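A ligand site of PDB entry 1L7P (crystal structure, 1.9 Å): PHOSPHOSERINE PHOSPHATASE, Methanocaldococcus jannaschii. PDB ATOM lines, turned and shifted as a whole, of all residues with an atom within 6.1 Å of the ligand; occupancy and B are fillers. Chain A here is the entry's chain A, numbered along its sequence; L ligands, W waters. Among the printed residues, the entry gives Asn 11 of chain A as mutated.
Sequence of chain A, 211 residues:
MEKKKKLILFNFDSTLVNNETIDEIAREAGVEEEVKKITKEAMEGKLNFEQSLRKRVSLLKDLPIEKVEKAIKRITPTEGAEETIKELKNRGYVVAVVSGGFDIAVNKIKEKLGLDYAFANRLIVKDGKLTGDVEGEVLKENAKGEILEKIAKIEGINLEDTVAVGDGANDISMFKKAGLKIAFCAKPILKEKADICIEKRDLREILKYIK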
ATOM      1  N   ASN A  11     -34.547  -9.673 -28.558  1.00  0.00           N
ATOM      2  CA  ASN A  11     -33.389  -9.207 -27.820  1.00  0.00           C
ATOM      3  C   ASN A  11     -33.021  -7.980 -28.654  1.00  0.00           C
ATOM      4  O   ASN A  11     -33.535  -7.825 -29.769  1.00  0.00           O
ATOM      5  CB  ASN A  11     -32.246 -10.232 -27.824  1.00  0.00           C
ATOM      6  CG  ASN A  11     -31.709 -10.487 -29.216  1.00  0.00           C
ATOM      7  OD1 ASN A  11     -32.353 -11.273 -29.949  1.00  0.00           O
ATOM      8  ND2 ASN A  11     -30.653  -9.907 -29.563  1.00  0.00           N
ATOM      9  N   PHE A  12     -32.150  -7.116 -28.144  1.00  0.00           N
ATOM     10  CA  PHE A  12     -31.780  -5.902 -28.868  1.00  0.00           C
ATOM     11  C   PHE A  12     -30.582  -6.058 -29.780  1.00  0.00           C
ATOM     12  O   PHE A  12     -30.723  -6.062 -30.998  1.00  0.00           O
ATOM     13  CB  PHE A  12     -31.544  -4.771 -27.863  1.00  0.00           C
ATOM     14  CG  PHE A  12     -31.193  -3.440 -28.496  1.00  0.00           C
ATOM     15  CD1 PHE A  12     -32.143  -2.719 -29.213  1.00  0.00           C
ATOM     16  CD2 PHE A  12     -29.937  -2.877 -28.306  1.00  0.00           C
ATOM     17  CE1 PHE A  12     -31.838  -1.451 -29.724  1.00  0.00           C
ATOM     18  CE2 PHE A  12     -29.623  -1.610 -28.812  1.00  0.00           C
ATOM     19  CZ  PHE A  12     -30.583  -0.904 -29.517  1.00  0.00           C
ATOM     20  N   ASP A  13     -29.386  -6.200 -29.202  1.00  0.00           N
ATOM     21  CA  ASP A  13     -28.162  -6.344 -29.980  1.00  0.00           C
ATOM     22  C   ASP A  13     -28.099  -7.516 -30.980  1.00  0.00           C
ATOM     23  O   ASP A  13     -28.334  -8.678 -30.623  1.00  0.00           O
ATOM     24  CB  ASP A  13     -26.960  -6.404 -29.030  1.00  0.00           C
ATOM     25  CG  ASP A  13     -26.866  -5.163 -28.139  1.00  0.00           C
ATOM     26  OD1 ASP A  13     -26.780  -4.048 -28.687  1.00  0.00           O
ATOM     27  OD2 ASP A  13     -26.875  -5.295 -26.895  1.00  0.00           O
ATOM     28  N   SER A  14     -27.801  -7.180 -32.236  1.00  0.00           N
ATOM     29  CA  SER A  14     -27.701  -8.140 -33.334  1.00  0.00           C
ATOM     30  C   SER A  14     -29.015  -8.746 -33.802  1.00  0.00           C
ATOM     31  O   SER A  14     -29.027  -9.600 -34.697  1.00  0.00           O
ATOM     32  CB  SER A  14     -26.717  -9.260 -32.978  1.00  0.00           C
ATOM     33  OG  SER A  14     -25.405  -8.750 -32.872  1.00  0.00           O
ATOM     34  N   THR A  15     -30.122  -8.321 -33.220  1.00  0.00           N
ATOM     35  CA  THR A  15     -31.421  -8.832 -33.618  1.00  0.00           C
ATOM     36  C   THR A  15     -32.255  -7.671 -34.135  1.00  0.00           C
ATOM     37  O   THR A  15     -32.532  -7.600 -35.327  1.00  0.00           O
ATOM     38  CB  THR A  15     -32.113  -9.550 -32.446  1.00  0.00           C
ATOM     39  OG1 THR A  15     -31.386 -10.745 -32.147  1.00  0.00           O
ATOM     40  CG2 THR A  15     -33.549  -9.916 -32.805  1.00  0.00           C
ATOM     41  N   GLU A  20     -23.482  -4.656 -31.679  1.00  0.00           N
ATOM     42  CA  GLU A  20     -23.403  -5.030 -30.278  1.00  0.00           C
ATOM     43  C   GLU A  20     -23.084  -3.710 -29.586  1.00  0.00           C
ATOM     44  O   GLU A  20     -21.958  -3.230 -29.662  1.00  0.00           O
ATOM     45  CB  GLU A  20     -22.263  -6.037 -30.041  1.00  0.00           C
ATOM     46  CG  GLU A  20     -22.520  -7.448 -30.563  1.00  0.00           C
ATOM     47  CD  GLU A  20     -23.686  -8.128 -29.861  1.00  0.00           C
ATOM     48  OE1 GLU A  20     -23.822  -7.966 -28.642  1.00  0.00           O
ATOM     49  OE2 GLU A  20     -24.452  -8.837 -30.533  1.00  0.00           O
ATOM     50  N   ILE A  22     -22.457  -2.732 -26.570  1.00  0.00           N
ATOM     51  CA  ILE A  22     -21.313  -2.768 -25.675  1.00  0.00           C
ATOM     52  C   ILE A  22     -19.999  -2.726 -26.451  1.00  0.00           C
ATOM     53  O   ILE A  22     -19.020  -2.133 -25.994  1.00  0.00           O
ATOM     54  CB  ILE A  22     -21.349  -4.024 -24.772  1.00  0.00           C
ATOM     55  CG1 ILE A  22     -20.173  -4.028 -23.807  1.00  0.00           C
ATOM     56  CG2 ILE A  22     -21.342  -5.274 -25.638  1.00  0.00           C
ATOM     57  CD1 ILE A  22     -20.126  -2.822 -22.884  1.00  0.00           C
ATOM     58  N   THR A  39     -17.694 -10.442 -25.264  1.00  0.00           N
ATOM     59  CA  THR A  39     -19.091 -10.449 -25.715  1.00  0.00           C
ATOM     60  C   THR A  39     -19.367 -11.757 -26.437  1.00  0.00           C
ATOM     61  O   THR A  39     -20.378 -12.422 -26.179  1.00  0.00           O
ATOM     62  CB  THR A  39     -19.361  -9.265 -26.669  1.00  0.00           C
ATOM     63  OG1 THR A  39     -19.271  -8.035 -25.947  1.00  0.00           O
ATOM     64  CG2 THR A  39     -20.745  -9.379 -27.277  1.00  0.00           C
ATOM     65  N   LYS A  40     -18.459 -12.143 -27.322  1.00  0.00           N
ATOM     66  CA  LYS A  40     -18.602 -13.373 -28.092  1.00  0.00           C
ATOM     67  C   LYS A  40     -18.734 -14.582 -27.159  1.00  0.00           C
ATOM     68  O   LYS A  40     -19.588 -15.444 -27.370  1.00  0.00           O
ATOM     69  CB  LYS A  40     -17.386 -13.550 -28.999  1.00  0.00           C
ATOM     70  CG  LYS A  40     -17.476 -14.724 -29.962  1.00  0.00           C
ATOM     71  CD  LYS A  40     -16.168 -14.912 -30.714  1.00  0.00           C
ATOM     72  CE  LYS A  40     -16.249 -16.051 -31.722  1.00  0.00           C
ATOM     73  NZ  LYS A  40     -17.189 -15.728 -32.841  1.00  0.00           N
ATOM     74  N   ALA A  42     -19.625 -14.556 -23.997  1.00  0.00           N
ATOM     75  CA  ALA A  42     -20.840 -14.405 -23.210  1.00  0.00           C
ATOM     76  C   ALA A  42     -22.046 -14.893 -23.989  1.00  0.00           C
ATOM     77  O   ALA A  42     -22.865 -15.658 -23.467  1.00  0.00           O
ATOM     78  CB  ALA A  42     -21.029 -12.941 -22.797  1.00  0.00           C
ATOM     79  N   MET A  43     -22.161 -14.464 -25.243  1.00  0.00           N
ATOM     80  CA  MET A  43     -23.294 -14.869 -26.068  1.00  0.00           C
ATOM     81  C   MET A  43     -23.229 -16.351 -26.456  1.00  0.00           C
ATOM     82  O   MET A  43     -24.252 -16.949 -26.743  1.00  0.00           O
ATOM     83  CB  MET A  43     -23.363 -14.012 -27.335  1.00  0.00           C
ATOM     84  CG  MET A  43     -23.740 -12.551 -27.058  1.00  0.00           C
ATOM     85  SD  MET A  43     -25.408 -12.326 -26.116  1.00  0.00           S
ATOM     86  CE  MET A  43     -24.742 -12.358 -24.319  1.00  0.00           C
ATOM     87  N   PHE A  49     -23.392 -14.447 -17.609  1.00  0.00           N
ATOM     88  CA  PHE A  49     -23.731 -13.138 -18.175  1.00  0.00           C
ATOM     89  C   PHE A  49     -23.427 -11.917 -17.304  1.00  0.00           C
ATOM     90  O   PHE A  49     -22.740 -10.987 -17.752  1.00  0.00           O
ATOM     91  CB  PHE A  49     -25.198 -13.057 -18.591  1.00  0.00           C
ATOM     92  CG  PHE A  49     -25.512 -11.782 -19.340  1.00  0.00           C
ATOM     93  CD1 PHE A  49     -25.078 -11.616 -20.657  1.00  0.00           C
ATOM     94  CD2 PHE A  49     -26.144 -10.728 -18.704  1.00  0.00           C
ATOM     95  CE1 PHE A  49     -25.268 -10.404 -21.312  1.00  0.00           C
ATOM     96  CE2 PHE A  49     -26.326  -9.508 -19.350  1.00  0.00           C
ATOM     97  CZ  PHE A  49     -25.884  -9.343 -20.662  1.00  0.00           C
ATOM     98  N   SER A  52     -19.704 -11.272 -16.937  1.00  0.00           N
ATOM     99  CA  SER A  52     -19.164 -10.825 -18.220  1.00  0.00           C
ATOM    100  C   SER A  52     -19.563  -9.390 -18.567  1.00  0.00           C
ATOM    101  O   SER A  52     -18.789  -8.678 -19.199  1.00  0.00           O
ATOM    102  CB  SER A  52     -19.618 -11.749 -19.367  1.00  0.00           C
ATOM    103  OG  SER A  52     -20.947 -11.450 -19.775  1.00  0.00           O
ATOM    104  N   LEU A  53     -20.762  -8.989 -18.165  1.00  0.00           N
ATOM    105  CA  LEU A  53     -21.214  -7.627 -18.460  1.00  0.00           C
ATOM    106  C   LEU A  53     -20.509  -6.634 -17.537  1.00  0.00           C
ATOM    107  O   LEU A  53     -20.057  -5.585 -17.982  1.00  0.00           O
ATOM    108  CB  LEU A  53     -22.731  -7.489 -18.301  1.00  0.00           C
ATOM    109  CG  LEU A  53     -23.277  -6.123 -18.731  1.00  0.00           C
ATOM    110  CD1 LEU A  53     -23.071  -5.939 -20.228  1.00  0.00           C
ATOM    111  CD2 LEU A  53     -24.754  -5.999 -18.388  1.00  0.00           C
ATOM    112  N   ARG A  56     -16.991  -6.221 -18.749  1.00  0.00           N
ATOM    113  CA  ARG A  56     -16.890  -5.391 -19.953  1.00  0.00           C
ATOM    114  C   ARG A  56     -17.166  -3.905 -19.664  1.00  0.00           C
ATOM    115  O   ARG A  56     -16.523  -3.037 -20.225  1.00  0.00           O
ATOM    116  CB  ARG A  56     -17.847  -5.903 -21.028  1.00  0.00           C
ATOM    117  CG  ARG A  56     -17.389  -7.198 -21.678  1.00  0.00           C
ATOM    118  CD  ARG A  56     -18.470  -7.739 -22.594  1.00  0.00           C
ATOM    119  NE  ARG A  56     -19.568  -8.347 -21.835  1.00  0.00           N
ATOM    120  CZ  ARG A  56     -20.730  -8.689 -22.368  1.00  0.00           C
ATOM    121  NH1 ARG A  56     -20.947  -8.484 -23.671  1.00  0.00           N
ATOM    122  NH2 ARG A  56     -21.677  -9.242 -21.615  1.00  0.00           N
ATOM    123  N   VAL A  98     -36.315  -6.854 -24.933  1.00  0.00           N
ATOM    124  CA  VAL A  98     -35.721  -7.147 -23.628  1.00  0.00           C
ATOM    125  C   VAL A  98     -34.234  -7.370 -23.889  1.00  0.00           C
ATOM    126  O   VAL A  98     -33.862  -8.286 -24.594  1.00  0.00           O
ATOM    127  CB  VAL A  98     -36.353  -8.413 -23.005  1.00  0.00           C
ATOM    128  CG1 VAL A  98     -35.741  -8.674 -21.628  1.00  0.00           C
ATOM    129  CG2 VAL A  98     -37.866  -8.236 -22.904  1.00  0.00           C
ATOM    130  N   SER A  99     -33.402  -6.525 -23.298  1.00  0.00           N
ATOM    131  CA  SER A  99     -31.975  -6.593 -23.566  1.00  0.00           C
ATOM    132  C   SER A  99     -31.022  -6.531 -22.397  1.00  0.00           C
ATOM    133  O   SER A  99     -31.254  -5.813 -21.399  1.00  0.00           O
ATOM    134  CB  SER A  99     -31.638  -5.450 -24.539  1.00  0.00           C
ATOM    135  OG  SER A  99     -30.247  -5.338 -24.752  1.00  0.00           O
ATOM    136  N   GLY A 100     -29.928  -7.271 -22.517  1.00  0.00           N
ATOM    137  CA  GLY A 100     -28.908  -7.256 -21.484  1.00  0.00           C
ATOM    138  C   GLY A 100     -28.112  -5.999 -21.740  1.00  0.00           C
ATOM    139  O   GLY A 100     -27.135  -5.720 -21.051  1.00  0.00           O
ATOM    140  N   GLY A 101     -28.537  -5.248 -22.754  1.00  0.00           N
ATOM    141  CA  GLY A 101     -27.894  -4.008 -23.129  1.00  0.00           C
ATOM    142  C   GLY A 101     -28.215  -2.830 -22.207  1.00  0.00           C
ATOM    143  O   GLY A 101     -28.591  -3.016 -21.047  1.00  0.00           O
ATOM    144  N   VAL A 138     -31.760  -7.114 -15.973  1.00  0.00           N
ATOM    145  CA  VAL A 138     -31.582  -8.004 -17.108  1.00  0.00           C
ATOM    146  C   VAL A 138     -30.148  -8.539 -16.993  1.00  0.00           C
ATOM    147  O   VAL A 138     -29.384  -8.544 -17.957  1.00  0.00           O
ATOM    148  CB  VAL A 138     -31.777  -7.265 -18.462  1.00  0.00           C
ATOM    149  CG1 VAL A 138     -32.109  -8.284 -19.577  1.00  0.00           C
ATOM    150  CG2 VAL A 138     -32.906  -6.258 -18.331  1.00  0.00           C
ATOM    151  N   LYS A 144     -34.534 -12.561 -18.418  1.00  0.00           N
ATOM    152  CA  LYS A 144     -35.476 -12.340 -19.513  1.00  0.00           C
ATOM    153  C   LYS A 144     -36.753 -13.155 -19.408  1.00  0.00           C
ATOM    154  O   LYS A 144     -37.827 -12.709 -19.821  1.00  0.00           O
ATOM    155  CB  LYS A 144     -34.773 -12.574 -20.864  1.00  0.00           C
ATOM    156  CG  LYS A 144     -33.596 -11.627 -21.110  1.00  0.00           C
ATOM    157  CD  LYS A 144     -33.262 -11.519 -22.601  1.00  0.00           C
ATOM    158  CE  LYS A 144     -32.045 -10.643 -22.848  1.00  0.00           C
ATOM    159  NZ  LYS A 144     -31.756 -10.433 -24.306  1.00  0.00           N
ATOM    160  N   ASP A 167     -30.842 -14.371 -29.924  1.00  0.00           N
ATOM    161  CA  ASP A 167     -29.651 -14.768 -30.640  1.00  0.00           C
ATOM    162  C   ASP A 167     -28.466 -15.164 -29.763  1.00  0.00           C
ATOM    163  O   ASP A 167     -27.431 -15.578 -30.263  1.00  0.00           O
ATOM    164  CB  ASP A 167     -29.236 -13.651 -31.609  1.00  0.00           C
ATOM    165  CG  ASP A 167     -28.704 -12.416 -30.897  1.00  0.00           C
ATOM    166  OD1 ASP A 167     -28.827 -12.323 -29.656  1.00  0.00           O
ATOM    167  OD2 ASP A 167     -28.156 -11.534 -31.590  1.00  0.00           O
ATOM    168  N   GLY A 168     -28.632 -15.066 -28.449  1.00  0.00           N
ATOM    169  CA  GLY A 168     -27.521 -15.413 -27.577  1.00  0.00           C
ATOM    170  C   GLY A 168     -27.882 -16.229 -26.349  1.00  0.00           C
ATOM    171  O   GLY A 168     -29.054 -16.519 -26.084  1.00  0.00           O
ATOM    172  N   ASN A 170     -27.974 -15.457 -23.254  1.00  0.00           N
ATOM    173  CA  ASN A 170     -28.848 -14.823 -22.281  1.00  0.00           C
ATOM    174  C   ASN A 170     -30.303 -14.729 -22.734  1.00  0.00           C
ATOM    175  O   ASN A 170     -31.148 -14.123 -22.064  1.00  0.00           O
ATOM    176  CB  ASN A 170     -28.307 -13.435 -21.882  1.00  0.00           C
ATOM    177  CG  ASN A 170     -28.391 -12.416 -22.999  1.00  0.00           C
ATOM    178  OD1 ASN A 170     -28.185 -12.735 -24.168  1.00  0.00           O
ATOM    179  ND2 ASN A 170     -28.669 -11.164 -22.634  1.00  0.00           N
ATOM    180  N   ASP A 171     -30.613 -15.346 -23.886  1.00  0.00           N
ATOM    181  CA  ASP A 171     -31.985 -15.389 -24.385  1.00  0.00           C
ATOM    182  C   ASP A 171     -32.576 -16.757 -24.061  1.00  0.00           C
ATOM    183  O   ASP A 171     -33.729 -17.044 -24.368  1.00  0.00           O
ATOM    184  CB  ASP A 171     -32.023 -15.156 -25.898  1.00  0.00           C
ATOM    185  CG  ASP A 171     -31.600 -13.754 -26.270  1.00  0.00           C
ATOM    186  OD1 ASP A 171     -32.097 -12.809 -25.623  1.00  0.00           O
ATOM    187  OD2 ASP A 171     -30.787 -13.596 -27.205  1.00  0.00           O
HETATM  188  N1  LIG L   1     -25.279  -8.710 -26.743  1.00  0.00           N
HETATM  189  C1  LIG L   1     -25.285  -8.078 -25.416  1.00  0.00           C
HETATM  190  C2  LIG L   1     -26.669  -8.239 -24.780  1.00  0.00           C
HETATM  191  O1  LIG L   1     -27.695  -7.658 -25.573  1.00  0.00           O
HETATM  192  C3  LIG L   1     -24.223  -8.711 -24.518  1.00  0.00           C
HETATM  193  O2  LIG L   1     -23.344  -9.411 -25.050  1.00  0.00           O
HETATM  194  O3  LIG L   1     -24.119  -8.272 -23.352  1.00  0.00           O
HETATM  195  P1  LIG L   1     -28.980  -8.344 -25.913  1.00  0.00           P
HETATM  196  O4  LIG L   1     -28.741  -9.330 -26.993  1.00  0.00           O
HETATM  197  O5  LIG L   1     -29.964  -7.335 -26.385  1.00  0.00           O
HETATM  198  O6  LIG L   1     -29.510  -9.027 -24.711  1.00  0.00           O
HETATM  199  O   HOH W   1     -28.872 -11.746 -26.502  1.00  0.00           O
HETATM  200  O   HOH W   2     -24.725  -5.679 -23.122  1.00  0.00           O
HETATM  201  O   HOH W   3     -26.579 -10.266 -28.860  1.00  0.00           O
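Water W2 bridges an oxygen (O3) of the ligand (2.7 Å) and the backbone carbonyl oxygen of Gly 100 (3.2 Å).
OG of Ser 99 is in hydrogen-bond range of N of Gly 101, 2.6 Å away.
The backbone carbonyl oxygen (O) of Val 98 sits at hydrogen-bond distance from the side-chain amino group (NZ) of Lys 144, 3.0 Å away.
NZ of Lys 144 lies within salt-bridge range of OD1 of Asp 171 (2.7 Å).
O of Asp 13 sits at hydrogen-bond distance from ND2 of Asn 11 (2.8 Å).
The guanidinium group (NH1) of Arg 56 lies within hydrogen-bond range of the side-chain hydroxyl (OG1) of Thr 39, 2.9 Å away.
The side-chain amide oxygen of Asn 170 lies close to the side-chain sulfur of Met 43 (3.4 Å).
The backbone carbonyl oxygen (O) of Phe 49 lies within hydrogen-bond range of the side-chain hydroxyl (OG) of Ser 52 (2.7 Å).
The side-chain amide nitrogen (ND2) of Asn 11 sits at hydrogen-bond distance from the side-chain carboxylate (OD1) of Asp 167, at 3.0 Å.
Thr 39 touches the ligand.
Phe 49 touches the ligand.
N of Gly 101 touches O1 of the ligand, 3.8 Å away.
Along chain A the residues within 4 Å of the ligand span positions 11 to 170.
The nearest printed residue that does not touch the ligand is Asp 167 (4.01 Å).
The side-chain carboxylate (OE1) of Glu 20 is in salt-bridge range of a nitrogen (N1) of the ligand (2.5 Å).
OG of Ser 99 lies within hydrogen-bond range of O5 of the ligand (2.6 Å).
An oxygen (O6) of the ligand is in salt-bridge range of the side-chain amino group (NZ) of Lys 144 (2.7 Å).
The backbone NH (N) of Phe 12 sits at hydrogen-bond distance from an oxygen (O5) of the ligand, 2.8 Å away.
The backbone NH of Asp 13 is in hydrogen-bond range of an oxygen (O5) of the ligand, at 3.1 Å.
A nitrogen (N1) of the ligand is in salt-bridge range of the side-chain carboxylate (OD2) of Asp 13 (3.8 Å).
N of Gly 100 is in hydrogen-bond range of O6 of the ligand (2.8 Å).
An oxygen (O2) of the ligand lies within salt-bridge range of the guanidinium group (NH1) of Arg 56, at 2.9 Å.
The side-chain amide nitrogen of Asn 170 lies within hydrogen-bond range of an oxygen (O6) of the ligand (3.1 Å).
ND2 of Asn 11 lies within hydrogen-bond range of O4 of the ligand, 3.3 Å away.
The side-chain sulfur of Met 43 sits at hydrogen-bond distance from a nitrogen (N1) of the ligand (3.7 Å).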
